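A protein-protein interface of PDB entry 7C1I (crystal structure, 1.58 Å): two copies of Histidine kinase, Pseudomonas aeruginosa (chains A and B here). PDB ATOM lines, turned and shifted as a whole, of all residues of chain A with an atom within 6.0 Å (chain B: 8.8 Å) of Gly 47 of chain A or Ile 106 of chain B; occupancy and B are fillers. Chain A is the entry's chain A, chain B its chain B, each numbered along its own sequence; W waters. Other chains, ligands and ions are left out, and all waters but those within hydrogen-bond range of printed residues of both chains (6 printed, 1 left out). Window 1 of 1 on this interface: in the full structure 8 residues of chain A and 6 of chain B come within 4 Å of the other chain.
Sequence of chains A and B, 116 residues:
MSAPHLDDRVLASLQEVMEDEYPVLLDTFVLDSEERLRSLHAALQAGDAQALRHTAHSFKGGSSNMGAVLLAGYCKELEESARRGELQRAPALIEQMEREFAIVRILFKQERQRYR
O of Gln 45 of chain A lies within hydrogen-bond range of NH1 of Arg 105 of chain B, 2.9 Å away. The backbone carbonyl oxygen (O) of Gly 47 of chain A lies within hydrogen-bond range of the side-chain amide nitrogen (NE2) of Gln 113 of chain B (2.9 Å).
OE2 of Glu 34 of chain B lies within salt-bridge range of NE of Arg 105 of chain B. The backbone carbonyl oxygen (O) of Lys 109 of chain B lies close to the side-chain amide nitrogen (NE2) of Gln 113 of chain B (3.5 Å).
Among the printed residues, pairs that only touch across the chains: Leu 44 of chain A with Ile 106 of chain B (3.5 Å), Ala 46 of chain A with Gln 113 of chain B (3.7 Å), Gly 47 of chain A with Ile 106 of chain B (3.1 Å), Leu 87 of chain A with Ile 106 of chain B (3.5 Å), Leu 87 of chain A with Gln 110 of chain B (3.7 Å), Gln 88 of chain A with Ile 103 of chain B (3.7 Å) and Pro 91 of chain A with Ala 102 of chain B (3.7 Å).
Ile 106 of chain B touches three residues of chain A. Of chain B, only Gln 113 comes within 4 Å of Ala 46 of chain A. Of the printed residues of chain B, Leu 44 of chain A touches Ile 106. Printed residues of chain B within 4 Å of Gln 88 of chain A: Ile 103 (3.7 Å). Of the printed residues of chain A, Gln 110 of chain B touches Leu 87. Of the printed residues of chain A, Gln 113 of chain B touches Ala 46 and Gly 47. Of the printed residues of chain A, Ile 103 of chain B touches Gln 88 (3.7 Å). Ala 43 of chain A touches none of the printed residues of chain B. The nearest residue of chain A that does not touch Ile 106 of chain B is Pro 91 of chain A (4.2 Å).
Printed residues of chain B that touch a printed residue of chain A: Ala 102, Ile 103, Arg 105, Ile 106, Gln 110 and Gln 113. Hydrophobic or aromatic side chains of chain B within 4 Å of the printed part of chain A: Ala 102, Ile 103 and Ile 106. Along chain B the printed residues that touch a printed residue of chain A span positions 102 to 113. Printed residues of chain A that touch a printed residue of chain B: Leu 44, Gln 45, Ala 46, Gly 47, Leu 87, Gln 88 and Pro 91. Among the printed residues, 9 pairs touch across the chains.
No position is printed for both chains.
Water W5 lies within hydrogen-bond range of the side-chain amide oxygen of Gln 110 of chain B (2.7 Å), the backbone NH of Leu 87 of chain A (2.8 Å) and the side-chain amide oxygen of Gln 88 of chain A (2.9 Å). Water W4 lies within hydrogen-bond range of the backbone carbonyl oxygen of Gln 45 of chain A (2.8 Å), the guanidinium group of Arg 105 of chain B (3.0 Å) and the side-chain amino group of Lys 109 of chain B (3.3 Å). Water W2 bridges O of Pro 91 of chain A and NH2 of Arg 99 of chain B. Water W6 bridges the guanidinium group of Arg 105 of chain B and the backbone carbonyl oxygen of Leu 44 of chain A. Water W1 bridges the side-chain carboxylate of Glu 34 of chain B (3.1 Å) and the side-chain amide nitrogen of Gln 45 of chain A (3.4 Å). Water W3 bridges NE2 of His 5 of chain B (3.3 Å) and O of Gln 88 of chain A (3.5 Å).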
ATOM      1  N   ALA A  42     -16.115  16.863  -5.791  1.00  0.00           N
ATOM      2  CA  ALA A  42     -15.702  17.616  -4.584  1.00  0.00           C
ATOM      3  C   ALA A  42     -14.183  17.439  -4.478  1.00  0.00           C
ATOM      4  O   ALA A  42     -13.476  18.434  -4.215  1.00  0.00           O
ATOM      5  CB  ALA A  42     -16.388  17.033  -3.372  1.00  0.00           C
ATOM      6  N   ALA A  43     -13.626  16.261  -4.774  1.00  0.00           N
ATOM      7  CA  ALA A  43     -12.173  16.008  -4.635  1.00  0.00           C
ATOM      8  C   ALA A  43     -11.476  16.870  -5.694  1.00  0.00           C
ATOM      9  O   ALA A  43     -10.356  17.386  -5.502  1.00  0.00           O
ATOM     10  CB  ALA A  43     -11.827  14.544  -4.740  1.00  0.00           C
ATOM     11  N   LEU A  44     -11.995  16.885  -6.927  1.00  0.00           N
ATOM     12  CA  LEU A  44     -11.385  17.679  -8.028  1.00  0.00           C
ATOM     13  C   LEU A  44     -11.366  19.159  -7.631  1.00  0.00           C
ATOM     14  O   LEU A  44     -10.301  19.792  -7.801  1.00  0.00           O
ATOM     15  CB  LEU A  44     -12.274  17.477  -9.258  1.00  0.00           C
ATOM     16  CG  LEU A  44     -11.672  18.233 -10.442  1.00  0.00           C
ATOM     17  CD1 LEU A  44     -10.336  17.646 -10.871  1.00  0.00           C
ATOM     18  CD2 LEU A  44     -12.666  18.233 -11.592  1.00  0.00           C
ATOM     19  N   GLN A  45     -12.432  19.668  -7.007  1.00  0.00           N
ATOM     20  CA  GLN A  45     -12.494  21.124  -6.703  1.00  0.00           C
ATOM     21  C   GLN A  45     -11.547  21.452  -5.542  1.00  0.00           C
ATOM     22  O   GLN A  45     -11.120  22.616  -5.420  1.00  0.00           O
ATOM     23  CB  GLN A  45     -13.931  21.549  -6.390  1.00  0.00           C
ATOM     24  CG  GLN A  45     -14.834  21.555  -7.614  1.00  0.00           C
ATOM     25  CD  GLN A  45     -14.352  22.324  -8.819  1.00  0.00           C
ATOM     26  OE1 GLN A  45     -13.884  21.787  -9.820  1.00  0.00           O
ATOM     27  NE2 GLN A  45     -14.455  23.636  -8.681  1.00  0.00           N
ATOM     28  N   ALA A  46     -11.232  20.448  -4.717  1.00  0.00           N
ATOM     29  CA  ALA A  46     -10.345  20.615  -3.541  1.00  0.00           C
ATOM     30  C   ALA A  46      -8.903  20.385  -4.006  1.00  0.00           C
ATOM     31  O   ALA A  46      -7.988  20.518  -3.167  1.00  0.00           O
ATOM     32  CB  ALA A  46     -10.799  19.723  -2.412  1.00  0.00           C
ATOM     33  N   GLY A  47      -8.575  19.933  -5.220  1.00  0.00           N
ATOM     34  CA  GLY A  47      -7.296  19.377  -5.705  1.00  0.00           C
ATOM     35  C   GLY A  47      -6.789  18.317  -4.744  1.00  0.00           C
ATOM     36  O   GLY A  47      -5.569  18.245  -4.487  1.00  0.00           O
ATOM     37  N   ASP A  48      -7.688  17.384  -4.418  1.00  0.00           N
ATOM     38  CA  ASP A  48      -7.293  16.243  -3.548  1.00  0.00           C
ATOM     39  C   ASP A  48      -6.974  14.962  -4.326  1.00  0.00           C
ATOM     40  O   ASP A  48      -7.903  14.175  -4.605  1.00  0.00           O
ATOM     41  CB  ASP A  48      -8.319  16.103  -2.424  1.00  0.00           C
ATOM     42  CG  ASP A  48      -7.978  15.158  -1.283  1.00  0.00           C
ATOM     43  OD1 ASP A  48      -7.093  14.325  -1.555  1.00  0.00           O
ATOM     44  OD2 ASP A  48      -8.743  15.196  -0.301  1.00  0.00           O
ATOM     45  N   ALA A  49      -5.704  14.699  -4.648  1.00  0.00           N
ATOM     46  CA  ALA A  49      -5.262  13.575  -5.508  1.00  0.00           C
ATOM     47  C   ALA A  49      -5.618  12.291  -4.750  1.00  0.00           C
ATOM     48  O   ALA A  49      -5.996  11.292  -5.394  1.00  0.00           O
ATOM     49  CB  ALA A  49      -3.799  13.574  -5.878  1.00  0.00           C
ATOM     50  N   LEU A  52      -9.324  11.566  -4.978  1.00  0.00           N
ATOM     51  CA  LEU A  52      -9.612  11.163  -6.381  1.00  0.00           C
ATOM     52  C   LEU A  52      -9.236   9.686  -6.544  1.00  0.00           C
ATOM     53  O   LEU A  52     -10.025   8.870  -7.061  1.00  0.00           O
ATOM     54  CB  LEU A  52      -8.903  12.010  -7.442  1.00  0.00           C
ATOM     55  CG  LEU A  52      -9.478  13.422  -7.547  1.00  0.00           C
ATOM     56  CD1 LEU A  52      -8.506  14.272  -8.349  1.00  0.00           C
ATOM     57  CD2 LEU A  52     -10.828  13.408  -8.247  1.00  0.00           C
ATOM     58  N   LEU A  87      -2.812  15.108 -12.439  1.00  0.00           N
ATOM     59  CA  LEU A  87      -4.234  15.527 -12.307  1.00  0.00           C
ATOM     60  C   LEU A  87      -4.729  16.272 -13.552  1.00  0.00           C
ATOM     61  O   LEU A  87      -5.956  16.495 -13.581  1.00  0.00           O
ATOM     62  CB  LEU A  87      -4.414  16.415 -11.072  1.00  0.00           C
ATOM     63  CG  LEU A  87      -4.033  15.746  -9.752  1.00  0.00           C
ATOM     64  CD1 LEU A  87      -4.346  16.628  -8.552  1.00  0.00           C
ATOM     65  CD2 LEU A  87      -4.643  14.355  -9.675  1.00  0.00           C
ATOM     66  N   GLN A  88      -3.926  16.423 -14.611  1.00  0.00           N
ATOM     67  CA  GLN A  88      -4.313  17.176 -15.834  1.00  0.00           C
ATOM     68  C   GLN A  88      -5.440  16.466 -16.593  1.00  0.00           C
ATOM     69  O   GLN A  88      -6.127  17.057 -17.449  1.00  0.00           O
ATOM     70  CB  GLN A  88      -3.129  17.377 -16.784  1.00  0.00           C
ATOM     71  CG  GLN A  88      -2.350  16.099 -17.061  1.00  0.00           C
ATOM     72  CD  GLN A  88      -1.269  15.742 -16.071  1.00  0.00           C
ATOM     73  OE1 GLN A  88      -1.123  16.312 -14.991  1.00  0.00           O
ATOM     74  NE2 GLN A  88      -0.500  14.744 -16.474  1.00  0.00           N
ATOM     75  N   ALA A  90      -7.806  14.635 -14.957  1.00  0.00           N
ATOM     76  CA  ALA A  90      -8.899  14.342 -14.002  1.00  0.00           C
ATOM     77  C   ALA A  90     -10.221  14.938 -14.481  1.00  0.00           C
ATOM     78  O   ALA A  90     -11.247  14.258 -14.491  1.00  0.00           O
ATOM     79  CB  ALA A  90      -8.628  14.579 -12.536  1.00  0.00           C
ATOM     80  N   PRO A  91     -10.253  16.234 -14.862  1.00  0.00           N
ATOM     81  CA  PRO A  91     -11.519  16.833 -15.288  1.00  0.00           C
ATOM     82  C   PRO A  91     -12.186  16.047 -16.425  1.00  0.00           C
ATOM     83  O   PRO A  91     -13.378  15.772 -16.382  1.00  0.00           O
ATOM     84  CB  PRO A  91     -11.127  18.251 -15.728  1.00  0.00           C
ATOM     85  CG  PRO A  91      -9.980  18.586 -14.807  1.00  0.00           C
ATOM     86  CD  PRO A  91      -9.213  17.279 -14.818  1.00  0.00           C
ATOM     87  N   HIS B   5      -0.799  22.836 -21.607  1.00  0.00           N
ATOM     88  CA  HIS B   5      -1.810  23.686 -20.922  1.00  0.00           C
ATOM     89  C   HIS B   5      -1.146  24.928 -20.315  1.00  0.00           C
ATOM     90  O   HIS B   5      -1.768  26.008 -20.322  1.00  0.00           O
ATOM     91  CB  HIS B   5      -2.531  22.872 -19.838  1.00  0.00           C
ATOM     92  CG  HIS B   5      -3.091  21.632 -20.452  1.00  0.00           C
ATOM     93  ND1 HIS B   5      -4.173  21.677 -21.308  1.00  0.00           N
ATOM     94  CD2 HIS B   5      -2.786  20.327 -20.288  1.00  0.00           C
ATOM     95  CE1 HIS B   5      -4.378  20.475 -21.808  1.00  0.00           C
ATOM     96  NE2 HIS B   5      -3.548  19.626 -21.182  1.00  0.00           N
ATOM     97  N   LEU B   6       0.010  24.693 -19.688  1.00  0.00           N
ATOM     98  CA  LEU B   6       0.728  25.805 -19.008  1.00  0.00           C
ATOM     99  C   LEU B   6       2.115  25.963 -19.641  1.00  0.00           C
ATOM    100  O   LEU B   6       2.778  24.958 -19.965  1.00  0.00           O
ATOM    101  CB  LEU B   6       0.849  25.556 -17.502  1.00  0.00           C
ATOM    102  CG  LEU B   6      -0.450  25.479 -16.702  1.00  0.00           C
ATOM    103  CD1 LEU B   6      -0.208  25.195 -15.228  1.00  0.00           C
ATOM    104  CD2 LEU B   6      -1.188  26.801 -16.852  1.00  0.00           C
ATOM    105  N   VAL B  30      -7.780  31.914 -10.383  1.00  0.00           N
ATOM    106  CA  VAL B  30      -8.921  30.948 -10.382  1.00  0.00           C
ATOM    107  C   VAL B  30     -10.193  31.771 -10.149  1.00  0.00           C
ATOM    108  O   VAL B  30     -11.230  31.547 -10.807  1.00  0.00           O
ATOM    109  CB  VAL B  30      -8.676  29.833  -9.345  1.00  0.00           C
ATOM    110  CG1 VAL B  30      -9.963  29.057  -9.102  1.00  0.00           C
ATOM    111  CG2 VAL B  30      -7.564  28.913  -9.826  1.00  0.00           C
ATOM    112  N   GLU B  34     -13.271  32.230 -12.919  1.00  0.00           N
ATOM    113  CA  GLU B  34     -14.616  31.686 -12.592  1.00  0.00           C
ATOM    114  C   GLU B  34     -15.580  32.842 -12.884  1.00  0.00           C
ATOM    115  O   GLU B  34     -16.680  32.564 -13.400  1.00  0.00           O
ATOM    116  CB  GLU B  34     -14.720  31.021 -11.220  1.00  0.00           C
ATOM    117  CG  GLU B  34     -13.950  29.712 -11.258  1.00  0.00           C
ATOM    118  CD  GLU B  34     -13.743  29.061  -9.902  1.00  0.00           C
ATOM    119  OE1 GLU B  34     -13.893  29.751  -8.875  1.00  0.00           O
ATOM    120  OE2 GLU B  34     -13.434  27.852  -9.939  1.00  0.00           O
ATOM    121  N   ARG B  99     -13.596  23.539 -20.307  1.00  0.00           N
ATOM    122  CA  ARG B  99     -12.862  22.254 -20.148  1.00  0.00           C
ATOM    123  C   ARG B  99     -11.363  22.535 -19.993  1.00  0.00           C
ATOM    124  O   ARG B  99     -10.507  21.768 -19.507  1.00  0.00           O
ATOM    125  CB  ARG B  99     -13.110  21.347 -21.358  1.00  0.00           C
ATOM    126  CG  ARG B  99     -14.566  20.919 -21.473  1.00  0.00           C
ATOM    127  CD  ARG B  99     -15.185  20.283 -20.242  1.00  0.00           C
ATOM    128  NE  ARG B  99     -15.635  21.082 -19.111  1.00  0.00           N
ATOM    129  CZ  ARG B  99     -15.362  20.888 -17.824  1.00  0.00           C
ATOM    130  NH1 ARG B  99     -15.750  21.833 -16.985  1.00  0.00           N
ATOM    131  NH2 ARG B  99     -14.798  19.825 -17.278  1.00  0.00           N
ATOM    132  N   GLU B 100     -10.878  23.577 -20.676  1.00  0.00           N
ATOM    133  CA  GLU B 100      -9.428  23.893 -20.571  1.00  0.00           C
ATOM    134  C   GLU B 100      -9.201  24.597 -19.229  1.00  0.00           C
ATOM    135  O   GLU B 100      -8.201  24.299 -18.542  1.00  0.00           O
ATOM    136  CB  GLU B 100      -9.030  24.822 -21.718  1.00  0.00           C
ATOM    137  CG  GLU B 100      -7.537  25.086 -21.655  1.00  0.00           C
ATOM    138  CD  GLU B 100      -6.583  23.915 -21.813  1.00  0.00           C
ATOM    139  OE1 GLU B 100      -6.966  22.876 -22.386  1.00  0.00           O
ATOM    140  OE2 GLU B 100      -5.407  24.113 -21.442  1.00  0.00           O
ATOM    141  N   PHE B 101     -10.063  25.510 -18.772  1.00  0.00           N
ATOM    142  CA  PHE B 101      -9.917  26.160 -17.443  1.00  0.00           C
ATOM    143  C   PHE B 101      -9.933  25.090 -16.346  1.00  0.00           C
ATOM    144  O   PHE B 101      -9.183  25.211 -15.361  1.00  0.00           O
ATOM    145  CB  PHE B 101     -10.969  27.250 -17.227  1.00  0.00           C
ATOM    146  CG  PHE B 101     -10.887  27.770 -15.815  1.00  0.00           C
ATOM    147  CD1 PHE B 101      -9.788  28.531 -15.450  1.00  0.00           C
ATOM    148  CD2 PHE B 101     -11.750  27.444 -14.784  1.00  0.00           C
ATOM    149  CE1 PHE B 101      -9.729  28.930 -14.124  1.00  0.00           C
ATOM    150  CE2 PHE B 101     -11.755  27.927 -13.486  1.00  0.00           C
ATOM    151  CZ  PHE B 101     -10.631  28.640 -13.127  1.00  0.00           C
ATOM    152  N   ALA B 102     -10.738  24.028 -16.464  1.00  0.00           N
ATOM    153  CA  ALA B 102     -10.776  23.027 -15.372  1.00  0.00           C
ATOM    154  C   ALA B 102      -9.381  22.402 -15.274  1.00  0.00           C
ATOM    155  O   ALA B 102      -9.013  22.043 -14.137  1.00  0.00           O
ATOM    156  CB  ALA B 102     -11.815  21.994 -15.736  1.00  0.00           C
ATOM    157  N   ILE B 103      -8.607  22.245 -16.350  1.00  0.00           N
ATOM    158  CA  ILE B 103      -7.234  21.658 -16.336  1.00  0.00           C
ATOM    159  C   ILE B 103      -6.387  22.669 -15.553  1.00  0.00           C
ATOM    160  O   ILE B 103      -5.613  22.337 -14.636  1.00  0.00           O
ATOM    161  CB  ILE B 103      -6.694  21.293 -17.731  1.00  0.00           C
ATOM    162  CG1 ILE B 103      -7.635  20.273 -18.380  1.00  0.00           C
ATOM    163  CG2 ILE B 103      -5.223  20.931 -17.600  1.00  0.00           C
ATOM    164  CD1 ILE B 103      -7.246  19.893 -19.787  1.00  0.00           C
ATOM    165  N   VAL B 104      -6.394  23.900 -16.075  1.00  0.00           N
ATOM    166  CA  VAL B 104      -5.538  24.939 -15.426  1.00  0.00           C
ATOM    167  C   VAL B 104      -5.851  25.004 -13.926  1.00  0.00           C
ATOM    168  O   VAL B 104      -4.964  25.129 -13.057  1.00  0.00           O
ATOM    169  CB  VAL B 104      -5.743  26.287 -16.143  1.00  0.00           C
ATOM    170  CG1 VAL B 104      -4.959  27.375 -15.421  1.00  0.00           C
ATOM    171  CG2 VAL B 104      -5.244  26.155 -17.572  1.00  0.00           C
ATOM    172  N   ARG B 105      -7.129  25.052 -13.541  1.00  0.00           N
ATOM    173  CA  ARG B 105      -7.640  25.131 -12.148  1.00  0.00           C
ATOM    174  C   ARG B 105      -6.958  24.000 -11.371  1.00  0.00           C
ATOM    175  O   ARG B 105      -6.434  24.284 -10.277  1.00  0.00           O
ATOM    176  CB  ARG B 105      -9.168  25.092 -12.052  1.00  0.00           C
ATOM    177  CG  ARG B 105      -9.615  25.478 -10.650  1.00  0.00           C
ATOM    178  CD  ARG B 105     -11.111  25.234 -10.585  1.00  0.00           C
ATOM    179  NE  ARG B 105     -11.690  25.731  -9.348  1.00  0.00           N
ATOM    180  CZ  ARG B 105     -11.593  25.225  -8.124  1.00  0.00           C
ATOM    181  NH1 ARG B 105     -10.899  24.114  -7.942  1.00  0.00           N
ATOM    182  NH2 ARG B 105     -12.180  25.828  -7.106  1.00  0.00           N
ATOM    183  N   ILE B 106      -7.096  22.739 -11.794  1.00  0.00           N
ATOM    184  CA  ILE B 106      -6.576  21.689 -10.865  1.00  0.00           C
ATOM    185  C   ILE B 106      -5.053  21.828 -10.788  1.00  0.00           C
ATOM    186  O   ILE B 106      -4.485  21.527  -9.718  1.00  0.00           O
ATOM    187  CB  ILE B 106      -7.093  20.298 -11.284  1.00  0.00           C
ATOM    188  CG1 ILE B 106      -6.645  19.247 -10.264  1.00  0.00           C
ATOM    189  CG2 ILE B 106      -6.559  19.841 -12.631  1.00  0.00           C
ATOM    190  CD1 ILE B 106      -6.983  19.457  -8.810  1.00  0.00           C
ATOM    191  N   LEU B 107      -4.352  22.183 -11.870  1.00  0.00           N
ATOM    192  CA  LEU B 107      -2.869  22.304 -11.862  1.00  0.00           C
ATOM    193  C   LEU B 107      -2.529  23.425 -10.872  1.00  0.00           C
ATOM    194  O   LEU B 107      -1.506  23.329 -10.164  1.00  0.00           O
ATOM    195  CB  LEU B 107      -2.325  22.550 -13.272  1.00  0.00           C
ATOM    196  CG  LEU B 107      -2.448  21.356 -14.219  1.00  0.00           C
ATOM    197  CD1 LEU B 107      -1.934  21.791 -15.580  1.00  0.00           C
ATOM    198  CD2 LEU B 107      -1.553  20.239 -13.702  1.00  0.00           C
ATOM    199  N   PHE B 108      -3.335  24.490 -10.867  1.00  0.00           N
ATOM    200  CA  PHE B 108      -3.000  25.646  -9.993  1.00  0.00           C
ATOM    201  C   PHE B 108      -3.348  25.258  -8.551  1.00  0.00           C
ATOM    202  O   PHE B 108      -2.616  25.695  -7.639  1.00  0.00           O
ATOM    203  CB  PHE B 108      -3.758  26.913 -10.397  1.00  0.00           C
ATOM    204  CG  PHE B 108      -3.076  27.681 -11.501  1.00  0.00           C
ATOM    205  CD1 PHE B 108      -2.107  27.168 -12.349  1.00  0.00           C
ATOM    206  CD2 PHE B 108      -3.595  28.944 -11.731  1.00  0.00           C
ATOM    207  CE1 PHE B 108      -1.474  27.929 -13.318  1.00  0.00           C
ATOM    208  CE2 PHE B 108      -2.950  29.702 -12.696  1.00  0.00           C
ATOM    209  CZ  PHE B 108      -1.984  29.190 -13.529  1.00  0.00           C
ATOM    210  N   LYS B 109      -4.368  24.428  -8.307  1.00  0.00           N
ATOM    211  CA  LYS B 109      -4.682  24.027  -6.909  1.00  0.00           C
ATOM    212  C   LYS B 109      -3.552  23.113  -6.422  1.00  0.00           C
ATOM    213  O   LYS B 109      -3.064  23.270  -5.285  1.00  0.00           O
ATOM    214  CB  LYS B 109      -5.956  23.180  -6.833  1.00  0.00           C
ATOM    215  CG  LYS B 109      -7.183  24.054  -7.048  1.00  0.00           C
ATOM    216  CD  LYS B 109      -7.513  24.931  -5.859  1.00  0.00           C
ATOM    217  CE  LYS B 109      -8.677  25.882  -6.047  1.00  0.00           C
ATOM    218  NZ  LYS B 109      -8.925  26.615  -4.783  1.00  0.00           N
ATOM    219  N   GLN B 110      -3.064  22.256  -7.323  1.00  0.00           N
ATOM    220  CA  GLN B 110      -1.931  21.366  -6.949  1.00  0.00           C
ATOM    221  C   GLN B 110      -0.735  22.249  -6.576  1.00  0.00           C
ATOM    222  O   GLN B 110      -0.039  21.988  -5.575  1.00  0.00           O
ATOM    223  CB  GLN B 110      -1.685  20.379  -8.092  1.00  0.00           C
ATOM    224  CG  GLN B 110      -0.593  19.343  -7.875  1.00  0.00           C
ATOM    225  CD  GLN B 110      -0.582  18.418  -9.066  1.00  0.00           C
ATOM    226  OE1 GLN B 110      -0.455  18.865 -10.204  1.00  0.00           O
ATOM    227  NE2 GLN B 110      -0.669  17.127  -8.786  1.00  0.00           N
ATOM    228  N   GLU B 111      -0.370  23.180  -7.462  1.00  0.00           N
ATOM    229  CA  GLU B 111       0.817  24.052  -7.254  1.00  0.00           C
ATOM    230  C   GLU B 111       0.606  24.866  -5.971  1.00  0.00           C
ATOM    231  O   GLU B 111       1.537  25.081  -5.167  1.00  0.00           O
ATOM    232  CB  GLU B 111       0.982  25.000  -8.443  1.00  0.00           C
ATOM    233  CG  GLU B 111       2.123  25.994  -8.319  1.00  0.00           C
ATOM    234  CD  GLU B 111       3.513  25.472  -8.635  1.00  0.00           C
ATOM    235  OE1 GLU B 111       3.691  24.238  -8.629  1.00  0.00           O
ATOM    236  OE2 GLU B 111       4.311  26.344  -9.035  1.00  0.00           O
ATOM    237  N   ARG B 112      -0.586  25.406  -5.699  1.00  0.00           N
ATOM    238  CA  ARG B 112      -0.834  26.284  -4.524  1.00  0.00           C
ATOM    239  C   ARG B 112      -0.564  25.530  -3.217  1.00  0.00           C
ATOM    240  O   ARG B 112      -0.188  26.177  -2.220  1.00  0.00           O
ATOM    241  CB  ARG B 112      -2.269  26.821  -4.528  1.00  0.00           C
ATOM    242  CG  ARG B 112      -2.747  27.683  -3.369  1.00  0.00           C
ATOM    243  CD  ARG B 112      -1.921  28.954  -3.321  1.00  0.00           C
ATOM    244  NE  ARG B 112      -2.314  29.721  -2.149  1.00  0.00           N
ATOM    245  CZ  ARG B 112      -1.732  29.576  -0.963  1.00  0.00           C
ATOM    246  NH1 ARG B 112      -0.841  28.615  -0.786  1.00  0.00           N
ATOM    247  NH2 ARG B 112      -2.041  30.398   0.023  1.00  0.00           N
ATOM    248  N   GLN B 113      -0.744  24.208  -3.160  1.00  0.00           N
ATOM    249  CA  GLN B 113      -0.548  23.344  -1.964  1.00  0.00           C
ATOM    250  C   GLN B 113       0.942  23.419  -1.613  1.00  0.00           C
ATOM    251  O   GLN B 113       1.210  22.943  -0.491  1.00  0.00           O
ATOM    252  CB  GLN B 113      -1.159  21.966  -2.225  1.00  0.00           C
ATOM    253  CG  GLN B 113      -2.680  22.024  -2.203  1.00  0.00           C
ATOM    254  CD  GLN B 113      -3.173  20.716  -2.772  1.00  0.00           C
ATOM    255  OE1 GLN B 113      -2.369  19.858  -3.131  1.00  0.00           O
ATOM    256  NE2 GLN B 113      -4.348  20.691  -3.380  1.00  0.00           N
HETATM  257  O   HOH W   1     -15.705  26.774  -8.088  1.00  0.00           O
HETATM  258  O   HOH W   2     -15.190  17.443 -15.078  1.00  0.00           O
HETATM  259  O   HOH W   3      -4.782  16.615 -20.624  1.00  0.00           O
HETATM  260  O   HOH W   4     -11.749  25.036  -4.262  1.00  0.00           O
HETATM  261  O   HOH W   5      -0.838  17.130 -12.173  1.00  0.00           O
HETATM  262  O   HOH W   6      -9.729  22.051  -9.519  1.00  0.00           O
